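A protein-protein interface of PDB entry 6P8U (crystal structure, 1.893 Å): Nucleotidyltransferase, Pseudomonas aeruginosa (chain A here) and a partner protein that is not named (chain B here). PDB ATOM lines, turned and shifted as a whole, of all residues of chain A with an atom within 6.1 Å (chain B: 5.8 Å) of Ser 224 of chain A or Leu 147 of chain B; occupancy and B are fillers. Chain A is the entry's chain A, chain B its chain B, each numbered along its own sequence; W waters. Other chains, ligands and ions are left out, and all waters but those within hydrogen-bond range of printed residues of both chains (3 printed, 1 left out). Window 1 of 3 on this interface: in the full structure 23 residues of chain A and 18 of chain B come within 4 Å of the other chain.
The side-chain amide nitrogen (NE2) of Gln 145 of chain B sits at hydrogen-bond distance from the backbone carbonyl oxygen (O) of Cys 209 of chain A, at 2.9 Å. OH of Tyr 101 of chain B lies within hydrogen-bond range of OE2 of Glu 221 of chain A (2.7 Å). The side-chain hydroxyl (OG1) of Thr 228 of chain A sits at hydrogen-bond distance from the backbone carbonyl oxygen (O) of Ser 146 of chain B (3.0 Å). O of Ser 224 of chain A lies close to O of Ser 146 of chain B (3.2 Å).
NH1 of Arg 220 of chain A sits at hydrogen-bond distance from OE1 of Gln 223 of chain A (3.0 Å). O of Arg 220 of chain A lies within hydrogen-bond range of OG of Ser 224 of chain A, at 3.4 Å. The side-chain amide nitrogen (NE2) of Gln 223 of chain A sits at hydrogen-bond distance from the side-chain hydroxyl (OG) of Ser 271 of chain A (2.8 Å). The backbone carbonyl oxygen of Ser 224 of chain A is in hydrogen-bond range of the side-chain hydroxyl of Thr 228 of chain A, 2.9 Å away. The backbone NH (N) of Leu 147 of chain B lies within hydrogen-bond range of the backbone carbonyl oxygen (O) of Ala 160 of chain B (3.0 Å). The side-chain hydroxyl of Thr 150 of chain B is in hydrogen-bond range of the backbone carbonyl oxygen of Gly 148 of chain B (3.3 Å).
Among the printed residues, pairs that only touch across the chains: Arg 220 of chain A with Gln 98 of chain B, Arg 220 of chain A with Tyr 101 of chain B, Gln 223 of chain A with Gln 98 of chain B, Gln 223 of chain A with Leu 147 of chain B, Ser 224 of chain A with Leu 147 of chain B, Ala 227 of chain A with Ser 146 of chain B, Ala 227 of chain A with Leu 147 of chain B, Ala 227 of chain A with Gly 148 of chain B, Thr 228 of chain A with Gln 145 of chain B, Ser 267 of chain A with Gly 148 of chain B and Ser 271 of chain A with Ser 149 of chain B.
Ser 224 of chain A touches two residues of chain B. Of the printed residues of chain A, Gln 145 of chain B touches Cys 209 and Thr 228. Of the printed residues of chain A, Tyr 101 of chain B touches Arg 220 (3.6 Å) and Glu 221 (2.7 Å). The nearest residue of chain B that does not touch Ser 224 of chain A is Gly 148 of chain B (5.0 Å). The nearest residue of chain A that does not touch Leu 147 of chain B is Thr 228 of chain A (5.0 Å). The nearest printed residue of chain A that does not touch Gln 145 of chain B is Ser 224 of chain A (6.1 Å).
Of the 14 printed residues of chain B, 7 touch a printed residue of chain A. Of the 14 printed residues of chain A, 9 touch a printed residue of chain B. Hydrophobic or aromatic side chains of chain A that line the printed part of chain B: Ala 227. Among the printed residues, no Asp or Glu carboxylate lies within 4 Å of a Lys or Arg side-chain nitrogen of the other chain.
Water W2 bridges the backbone carbonyl oxygen (O) of Ser 149 of chain B (2.6 Å) and the side-chain amide nitrogen (NE2) of Gln 223 of chain A (2.9 Å). Water W3 lies within hydrogen-bond range of OG of Ser 267 of chain A (2.7 Å), OG of Ser 271 of chain A (2.9 Å) and N of Ser 149 of chain B (2.9 Å). Water W1 lies within hydrogen-bond range of O of Ser 146 of chain B (2.9 Å), NE2 of Gln 145 of chain B (3.2 Å) and OG1 of Thr 228 of chain A (3.2 Å).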
ATOM      1  N   CYS A 209      17.197  10.301 -35.064  1.00  0.00           N
ATOM      2  CA  CYS A 209      16.917  11.523 -34.310  1.00  0.00           C
ATOM      3  C   CYS A 209      15.837  11.313 -33.253  1.00  0.00           C
ATOM      4  O   CYS A 209      15.842  11.996 -32.221  1.00  0.00           O
ATOM      5  CB  CYS A 209      16.510  12.639 -35.270  1.00  0.00           C
ATOM      6  SG  CYS A 209      17.828  13.137 -36.406  1.00  0.00           S
ATOM      7  N   ASP A 219       4.203  17.278 -27.206  1.00  0.00           N
ATOM      8  CA  ASP A 219       4.806  18.597 -27.372  1.00  0.00           C
ATOM      9  C   ASP A 219       6.320  18.518 -27.267  1.00  0.00           C
ATOM     10  O   ASP A 219       7.033  19.119 -28.081  1.00  0.00           O
ATOM     11  CB  ASP A 219       4.236  19.575 -26.341  1.00  0.00           C
ATOM     12  CG  ASP A 219       4.386  19.073 -24.914  1.00  0.00           C
ATOM     13  OD1 ASP A 219       4.755  17.882 -24.721  1.00  0.00           O
ATOM     14  OD2 ASP A 219       4.146  19.873 -23.976  1.00  0.00           O
ATOM     15  N   ARG A 220       6.828  17.754 -26.292  1.00  0.00           N
ATOM     16  CA  ARG A 220       8.268  17.633 -26.121  1.00  0.00           C
ATOM     17  C   ARG A 220       8.893  16.790 -27.228  1.00  0.00           C
ATOM     18  O   ARG A 220       9.974  17.123 -27.736  1.00  0.00           O
ATOM     19  CB  ARG A 220       8.581  17.027 -24.754  1.00  0.00           C
ATOM     20  CG  ARG A 220       8.138  17.886 -23.595  1.00  0.00           C
ATOM     21  CD  ARG A 220       8.970  19.162 -23.535  1.00  0.00           C
ATOM     22  NE  ARG A 220       8.570  20.011 -22.412  1.00  0.00           N
ATOM     23  CZ  ARG A 220       8.977  21.262 -22.245  1.00  0.00           C
ATOM     24  NH1 ARG A 220       9.805  21.815 -23.137  1.00  0.00           N
ATOM     25  NH2 ARG A 220       8.549  21.960 -21.193  1.00  0.00           N
ATOM     26  N   GLU A 221       8.249  15.679 -27.597  1.00  0.00           N
ATOM     27  CA  GLU A 221       8.796  14.851 -28.668  1.00  0.00           C
ATOM     28  C   GLU A 221       8.883  15.636 -29.972  1.00  0.00           C
ATOM     29  O   GLU A 221       9.867  15.517 -30.723  1.00  0.00           O
ATOM     30  CB  GLU A 221       7.945  13.598 -28.853  1.00  0.00           C
ATOM     31  CG  GLU A 221       7.938  12.660 -27.653  1.00  0.00           C
ATOM     32  CD  GLU A 221       9.213  11.846 -27.532  1.00  0.00           C
ATOM     33  OE1 GLU A 221      10.006  11.834 -28.505  1.00  0.00           O
ATOM     34  OE2 GLU A 221       9.422  11.235 -26.459  1.00  0.00           O
ATOM     35  N   ILE A 222       7.878  16.470 -30.238  1.00  0.00           N
ATOM     36  CA  ILE A 222       7.869  17.262 -31.462  1.00  0.00           C
ATOM     37  C   ILE A 222       8.909  18.369 -31.386  1.00  0.00           C
ATOM     38  O   ILE A 222       9.665  18.599 -32.337  1.00  0.00           O
ATOM     39  CB  ILE A 222       6.459  17.824 -31.718  1.00  0.00           C
ATOM     40  CG1 ILE A 222       5.482  16.702 -32.131  1.00  0.00           C
ATOM     41  CG2 ILE A 222       6.516  18.953 -32.755  1.00  0.00           C
ATOM     42  CD1 ILE A 222       5.838  16.038 -33.455  1.00  0.00           C
ATOM     43  N   GLN A 223       8.953  19.082 -30.258  1.00  0.00           N
ATOM     44  CA  GLN A 223       9.945  20.136 -30.084  1.00  0.00           C
ATOM     45  C   GLN A 223      11.356  19.599 -30.299  1.00  0.00           C
ATOM     46  O   GLN A 223      12.157  20.200 -31.026  1.00  0.00           O
ATOM     47  CB  GLN A 223       9.817  20.759 -28.691  1.00  0.00           C
ATOM     48  CG  GLN A 223      10.865  21.842 -28.405  1.00  0.00           C
ATOM     49  CD  GLN A 223      10.811  22.345 -26.966  1.00  0.00           C
ATOM     50  OE1 GLN A 223      10.591  21.574 -26.029  1.00  0.00           O
ATOM     51  NE2 GLN A 223      11.000  23.640 -26.790  1.00  0.00           N
ATOM     52  N   SER A 224      11.679  18.467 -29.668  1.00  0.00           N
ATOM     53  CA  SER A 224      13.015  17.898 -29.813  1.00  0.00           C
ATOM     54  C   SER A 224      13.229  17.327 -31.208  1.00  0.00           C
ATOM     55  O   SER A 224      14.330  17.423 -31.755  1.00  0.00           O
ATOM     56  CB  SER A 224      13.251  16.813 -28.754  1.00  0.00           C
ATOM     57  OG  SER A 224      13.358  17.375 -27.446  1.00  0.00           O
ATOM     58  N   PHE A 225      12.201  16.707 -31.789  1.00  0.00           N
ATOM     59  CA  PHE A 225      12.330  16.147 -33.132  1.00  0.00           C
ATOM     60  C   PHE A 225      12.688  17.229 -34.146  1.00  0.00           C
ATOM     61  O   PHE A 225      13.612  17.052 -34.953  1.00  0.00           O
ATOM     62  CB  PHE A 225      11.032  15.440 -33.512  1.00  0.00           C
ATOM     63  CG  PHE A 225      11.122  14.601 -34.767  1.00  0.00           C
ATOM     64  CD1 PHE A 225      12.332  14.313 -35.350  1.00  0.00           C
ATOM     65  CD2 PHE A 225       9.965  14.097 -35.348  1.00  0.00           C
ATOM     66  CE1 PHE A 225      12.403  13.525 -36.499  1.00  0.00           C
ATOM     67  CE2 PHE A 225      10.018  13.329 -36.493  1.00  0.00           C
ATOM     68  CZ  PHE A 225      11.248  13.042 -37.074  1.00  0.00           C
ATOM     69  N   PHE A 226      11.990  18.371 -34.099  1.00  0.00           N
ATOM     70  CA  PHE A 226      12.309  19.472 -35.004  1.00  0.00           C
ATOM     71  C   PHE A 226      13.694  20.028 -34.710  1.00  0.00           C
ATOM     72  O   PHE A 226      14.479  20.304 -35.621  1.00  0.00           O
ATOM     73  CB  PHE A 226      11.262  20.599 -34.894  1.00  0.00           C
ATOM     74  CG  PHE A 226      10.053  20.390 -35.758  1.00  0.00           C
ATOM     75  CD1 PHE A 226      10.180  20.242 -37.132  1.00  0.00           C
ATOM     76  CD2 PHE A 226       8.785  20.359 -35.197  1.00  0.00           C
ATOM     77  CE1 PHE A 226       9.068  20.037 -37.923  1.00  0.00           C
ATOM     78  CE2 PHE A 226       7.662  20.169 -35.983  1.00  0.00           C
ATOM     79  CZ  PHE A 226       7.800  20.008 -37.350  1.00  0.00           C
ATOM     80  N   ALA A 227      14.003  20.232 -33.427  1.00  0.00           N
ATOM     81  CA  ALA A 227      15.300  20.797 -33.061  1.00  0.00           C
ATOM     82  C   ALA A 227      16.436  19.902 -33.535  1.00  0.00           C
ATOM     83  O   ALA A 227      17.465  20.396 -34.003  1.00  0.00           O
ATOM     84  CB  ALA A 227      15.391  21.001 -31.547  1.00  0.00           C
ATOM     85  N   THR A 228      16.246  18.577 -33.459  1.00  0.00           N
ATOM     86  CA  THR A 228      17.307  17.665 -33.888  1.00  0.00           C
ATOM     87  C   THR A 228      17.390  17.597 -35.411  1.00  0.00           C
ATOM     88  O   THR A 228      18.482  17.515 -35.981  1.00  0.00           O
ATOM     89  CB  THR A 228      17.072  16.279 -33.289  1.00  0.00           C
ATOM     90  OG1 THR A 228      17.017  16.362 -31.852  1.00  0.00           O
ATOM     91  CG2 THR A 228      18.187  15.325 -33.682  1.00  0.00           C
ATOM     92  N   LEU A 229      16.248  17.641 -36.093  1.00  0.00           N
ATOM     93  CA  LEU A 229      16.269  17.688 -37.551  1.00  0.00           C
ATOM     94  C   LEU A 229      17.050  18.897 -38.049  1.00  0.00           C
ATOM     95  O   LEU A 229      17.920  18.775 -38.922  1.00  0.00           O
ATOM     96  CB  LEU A 229      14.843  17.718 -38.093  1.00  0.00           C
ATOM     97  CG  LEU A 229      14.036  16.427 -38.050  1.00  0.00           C
ATOM     98  CD1 LEU A 229      12.627  16.652 -38.623  1.00  0.00           C
ATOM     99  CD2 LEU A 229      14.754  15.324 -38.804  1.00  0.00           C
ATOM    100  N   SER A 267      10.851  24.320 -34.807  1.00  0.00           N
ATOM    101  CA  SER A 267      11.240  24.083 -33.419  1.00  0.00           C
ATOM    102  C   SER A 267      10.914  25.285 -32.538  1.00  0.00           C
ATOM    103  O   SER A 267      10.465  25.132 -31.395  1.00  0.00           O
ATOM    104  CB  SER A 267      12.742  23.770 -33.340  1.00  0.00           C
ATOM    105  OG  SER A 267      13.165  23.807 -31.989  1.00  0.00           O
ATOM    106  N   SER A 271       8.276  25.644 -29.373  1.00  0.00           N
ATOM    107  CA  SER A 271       8.650  26.218 -28.087  1.00  0.00           C
ATOM    108  C   SER A 271       7.665  27.299 -27.673  1.00  0.00           C
ATOM    109  O   SER A 271       7.273  27.372 -26.508  1.00  0.00           O
ATOM    110  CB  SER A 271      10.071  26.783 -28.152  1.00  0.00           C
ATOM    111  OG  SER A 271      11.004  25.780 -28.528  1.00  0.00           O
ATOM    112  N   TRP B  77      26.493  18.011 -22.371  1.00  0.00           N
ATOM    113  CA  TRP B  77      25.400  18.950 -22.602  1.00  0.00           C
ATOM    114  C   TRP B  77      25.956  20.199 -23.271  1.00  0.00           C
ATOM    115  O   TRP B  77      26.822  20.878 -22.705  1.00  0.00           O
ATOM    116  CB  TRP B  77      24.694  19.306 -21.298  1.00  0.00           C
ATOM    117  CG  TRP B  77      23.882  18.170 -20.769  1.00  0.00           C
ATOM    118  CD1 TRP B  77      24.329  17.120 -20.016  1.00  0.00           C
ATOM    119  CD2 TRP B  77      22.479  17.959 -20.954  1.00  0.00           C
ATOM    120  NE1 TRP B  77      23.292  16.271 -19.727  1.00  0.00           N
ATOM    121  CE2 TRP B  77      22.144  16.764 -20.290  1.00  0.00           C
ATOM    122  CE3 TRP B  77      21.473  18.664 -21.619  1.00  0.00           C
ATOM    123  CZ2 TRP B  77      20.842  16.256 -20.268  1.00  0.00           C
ATOM    124  CZ3 TRP B  77      20.182  18.158 -21.598  1.00  0.00           C
ATOM    125  CH2 TRP B  77      19.880  16.969 -20.925  1.00  0.00           C
ATOM    126  N   GLN B  98      11.712  21.180 -19.792  1.00  0.00           N
ATOM    127  CA  GLN B  98      12.355  20.626 -20.979  1.00  0.00           C
ATOM    128  C   GLN B  98      13.527  19.727 -20.602  1.00  0.00           C
ATOM    129  O   GLN B  98      13.705  18.639 -21.173  1.00  0.00           O
ATOM    130  CB  GLN B  98      12.828  21.752 -21.894  1.00  0.00           C
ATOM    131  CG  GLN B  98      13.368  21.275 -23.240  1.00  0.00           C
ATOM    132  CD  GLN B  98      14.317  22.280 -23.870  1.00  0.00           C
ATOM    133  OE1 GLN B  98      15.312  22.681 -23.254  1.00  0.00           O
ATOM    134  NE2 GLN B  98      14.013  22.698 -25.096  1.00  0.00           N
ATOM    135  N   LEU B  99      14.327  20.160 -19.630  1.00  0.00           N
ATOM    136  CA  LEU B  99      15.505  19.393 -19.242  1.00  0.00           C
ATOM    137  C   LEU B  99      15.128  18.119 -18.498  1.00  0.00           C
ATOM    138  O   LEU B  99      15.784  17.081 -18.659  1.00  0.00           O
ATOM    139  CB  LEU B  99      16.414  20.270 -18.384  1.00  0.00           C
ATOM    140  CG  LEU B  99      16.872  21.581 -19.028  1.00  0.00           C
ATOM    141  CD1 LEU B  99      17.629  22.433 -18.030  1.00  0.00           C
ATOM    142  CD2 LEU B  99      17.700  21.294 -20.259  1.00  0.00           C
ATOM    143  N   TYR B 101      12.543  16.295 -18.991  1.00  0.00           N
ATOM    144  CA  TYR B 101      12.049  15.316 -19.957  1.00  0.00           C
ATOM    145  C   TYR B 101      13.204  14.663 -20.707  1.00  0.00           C
ATOM    146  O   TYR B 101      13.188  13.458 -20.963  1.00  0.00           O
ATOM    147  CB  TYR B 101      11.073  15.990 -20.926  1.00  0.00           C
ATOM    148  CG  TYR B 101      10.331  15.041 -21.836  1.00  0.00           C
ATOM    149  CD1 TYR B 101       9.138  14.459 -21.434  1.00  0.00           C
ATOM    150  CD2 TYR B 101      10.807  14.750 -23.105  1.00  0.00           C
ATOM    151  CE1 TYR B 101       8.452  13.588 -22.259  1.00  0.00           C
ATOM    152  CE2 TYR B 101      10.119  13.881 -23.944  1.00  0.00           C
ATOM    153  CZ  TYR B 101       8.947  13.301 -23.510  1.00  0.00           C
ATOM    154  OH  TYR B 101       8.260  12.439 -24.321  1.00  0.00           O
ATOM    155  N   ALA B 102      14.215  15.444 -21.070  1.00  0.00           N
ATOM    156  CA  ALA B 102      15.373  14.882 -21.755  1.00  0.00           C
ATOM    157  C   ALA B 102      16.214  14.028 -20.813  1.00  0.00           C
ATOM    158  O   ALA B 102      16.719  12.968 -21.204  1.00  0.00           O
ATOM    159  CB  ALA B 102      16.223  16.010 -22.350  1.00  0.00           C
ATOM    160  N   GLN B 145      21.608  14.980 -29.436  1.00  0.00           N
ATOM    161  CA  GLN B 145      20.165  15.150 -29.434  1.00  0.00           C
ATOM    162  C   GLN B 145      19.856  16.584 -29.020  1.00  0.00           C
ATOM    163  O   GLN B 145      20.299  17.037 -27.963  1.00  0.00           O
ATOM    164  CB  GLN B 145      19.482  14.162 -28.484  1.00  0.00           C
ATOM    165  CG  GLN B 145      19.783  12.700 -28.770  1.00  0.00           C
ATOM    166  CD  GLN B 145      19.143  12.195 -30.056  1.00  0.00           C
ATOM    167  OE1 GLN B 145      19.660  11.268 -30.689  1.00  0.00           O
ATOM    168  NE2 GLN B 145      18.010  12.779 -30.428  1.00  0.00           N
ATOM    169  N   SER B 146      19.108  17.295 -29.849  1.00  0.00           N
ATOM    170  CA  SER B 146      18.734  18.679 -29.580  1.00  0.00           C
ATOM    171  C   SER B 146      17.319  18.733 -29.009  1.00  0.00           C
ATOM    172  O   SER B 146      16.457  17.918 -29.353  1.00  0.00           O
ATOM    173  CB  SER B 146      18.817  19.522 -30.857  1.00  0.00           C
ATOM    174  OG  SER B 146      20.153  19.559 -31.350  1.00  0.00           O
ATOM    175  N   LEU B 147      17.090  19.704 -28.120  1.00  0.00           N
ATOM    176  CA  LEU B 147      15.827  19.800 -27.412  1.00  0.00           C
ATOM    177  C   LEU B 147      15.005  21.021 -27.783  1.00  0.00           C
ATOM    178  O   LEU B 147      13.825  21.058 -27.452  1.00  0.00           O
ATOM    179  CB  LEU B 147      16.071  19.835 -25.896  1.00  0.00           C
ATOM    180  CG  LEU B 147      17.039  18.801 -25.324  1.00  0.00           C
ATOM    181  CD1 LEU B 147      17.138  18.961 -23.808  1.00  0.00           C
ATOM    182  CD2 LEU B 147      16.609  17.401 -25.685  1.00  0.00           C
ATOM    183  N   GLY B 148      15.592  22.010 -28.440  1.00  0.00           N
ATOM    184  CA  GLY B 148      14.907  23.260 -28.708  1.00  0.00           C
ATOM    185  C   GLY B 148      15.353  24.361 -27.761  1.00  0.00           C
ATOM    186  O   GLY B 148      16.296  24.217 -26.976  1.00  0.00           O
ATOM    187  N   SER B 149      14.636  25.483 -27.830  1.00  0.00           N
ATOM    188  CA  SER B 149      15.004  26.674 -27.073  1.00  0.00           C
ATOM    189  C   SER B 149      14.805  26.410 -25.585  1.00  0.00           C
ATOM    190  O   SER B 149      13.672  26.285 -25.111  1.00  0.00           O
ATOM    191  CB  SER B 149      14.171  27.864 -27.533  1.00  0.00           C
ATOM    192  OG  SER B 149      14.451  28.995 -26.736  1.00  0.00           O
ATOM    193  N   THR B 150      15.907  26.333 -24.846  1.00  0.00           N
ATOM    194  CA  THR B 150      15.859  26.081 -23.413  1.00  0.00           C
ATOM    195  C   THR B 150      15.748  27.377 -22.617  1.00  0.00           C
ATOM    196  O   THR B 150      14.918  27.486 -21.708  1.00  0.00           O
ATOM    197  CB  THR B 150      17.104  25.302 -22.972  1.00  0.00           C
ATOM    198  OG1 THR B 150      17.271  24.142 -23.805  1.00  0.00           O
ATOM    199  CG2 THR B 150      16.966  24.865 -21.524  1.00  0.00           C
ATOM    200  N   ALA B 160      19.546  23.745 -25.590  1.00  0.00           N
ATOM    201  CA  ALA B 160      20.248  22.627 -24.984  1.00  0.00           C
ATOM    202  C   ALA B 160      20.216  21.391 -25.880  1.00  0.00           C
ATOM    203  O   ALA B 160      19.261  21.151 -26.622  1.00  0.00           O
ATOM    204  CB  ALA B 160      19.635  22.292 -23.625  1.00  0.00           C
ATOM    205  N   GLY B 161      21.292  20.619 -25.808  1.00  0.00           N
ATOM    206  CA  GLY B 161      21.368  19.330 -26.467  1.00  0.00           C
ATOM    207  C   GLY B 161      22.302  18.444 -25.674  1.00  0.00           C
ATOM    208  O   GLY B 161      23.124  18.929 -24.887  1.00  0.00           O
ATOM    209  N   TYR B 162      22.151  17.132 -25.866  1.00  0.00           N
ATOM    210  CA  TYR B 162      22.950  16.158 -25.135  1.00  0.00           C
ATOM    211  C   TYR B 162      23.478  15.084 -26.072  1.00  0.00           C
ATOM    212  O   TYR B 162      22.785  14.650 -26.997  1.00  0.00           O
ATOM    213  CB  TYR B 162      22.141  15.504 -23.984  1.00  0.00           C
ATOM    214  CG  TYR B 162      20.979  14.646 -24.421  1.00  0.00           C
ATOM    215  CD1 TYR B 162      21.161  13.305 -24.740  1.00  0.00           C
ATOM    216  CD2 TYR B 162      19.689  15.167 -24.490  1.00  0.00           C
ATOM    217  CE1 TYR B 162      20.102  12.514 -25.129  1.00  0.00           C
ATOM    218  CE2 TYR B 162      18.623  14.380 -24.887  1.00  0.00           C
ATOM    219  CZ  TYR B 162      18.833  13.053 -25.201  1.00  0.00           C
ATOM    220  OH  TYR B 162      17.766  12.270 -25.589  1.00  0.00           O
HETATM  221  O   HOH W   1      16.244  15.020 -28.996  1.00  0.00           O
HETATM  222  O   HOH W   2      11.275  25.342 -24.499  1.00  0.00           O
HETATM  223  O   HOH W   3      13.227  25.990 -30.333  1.00  0.00           O
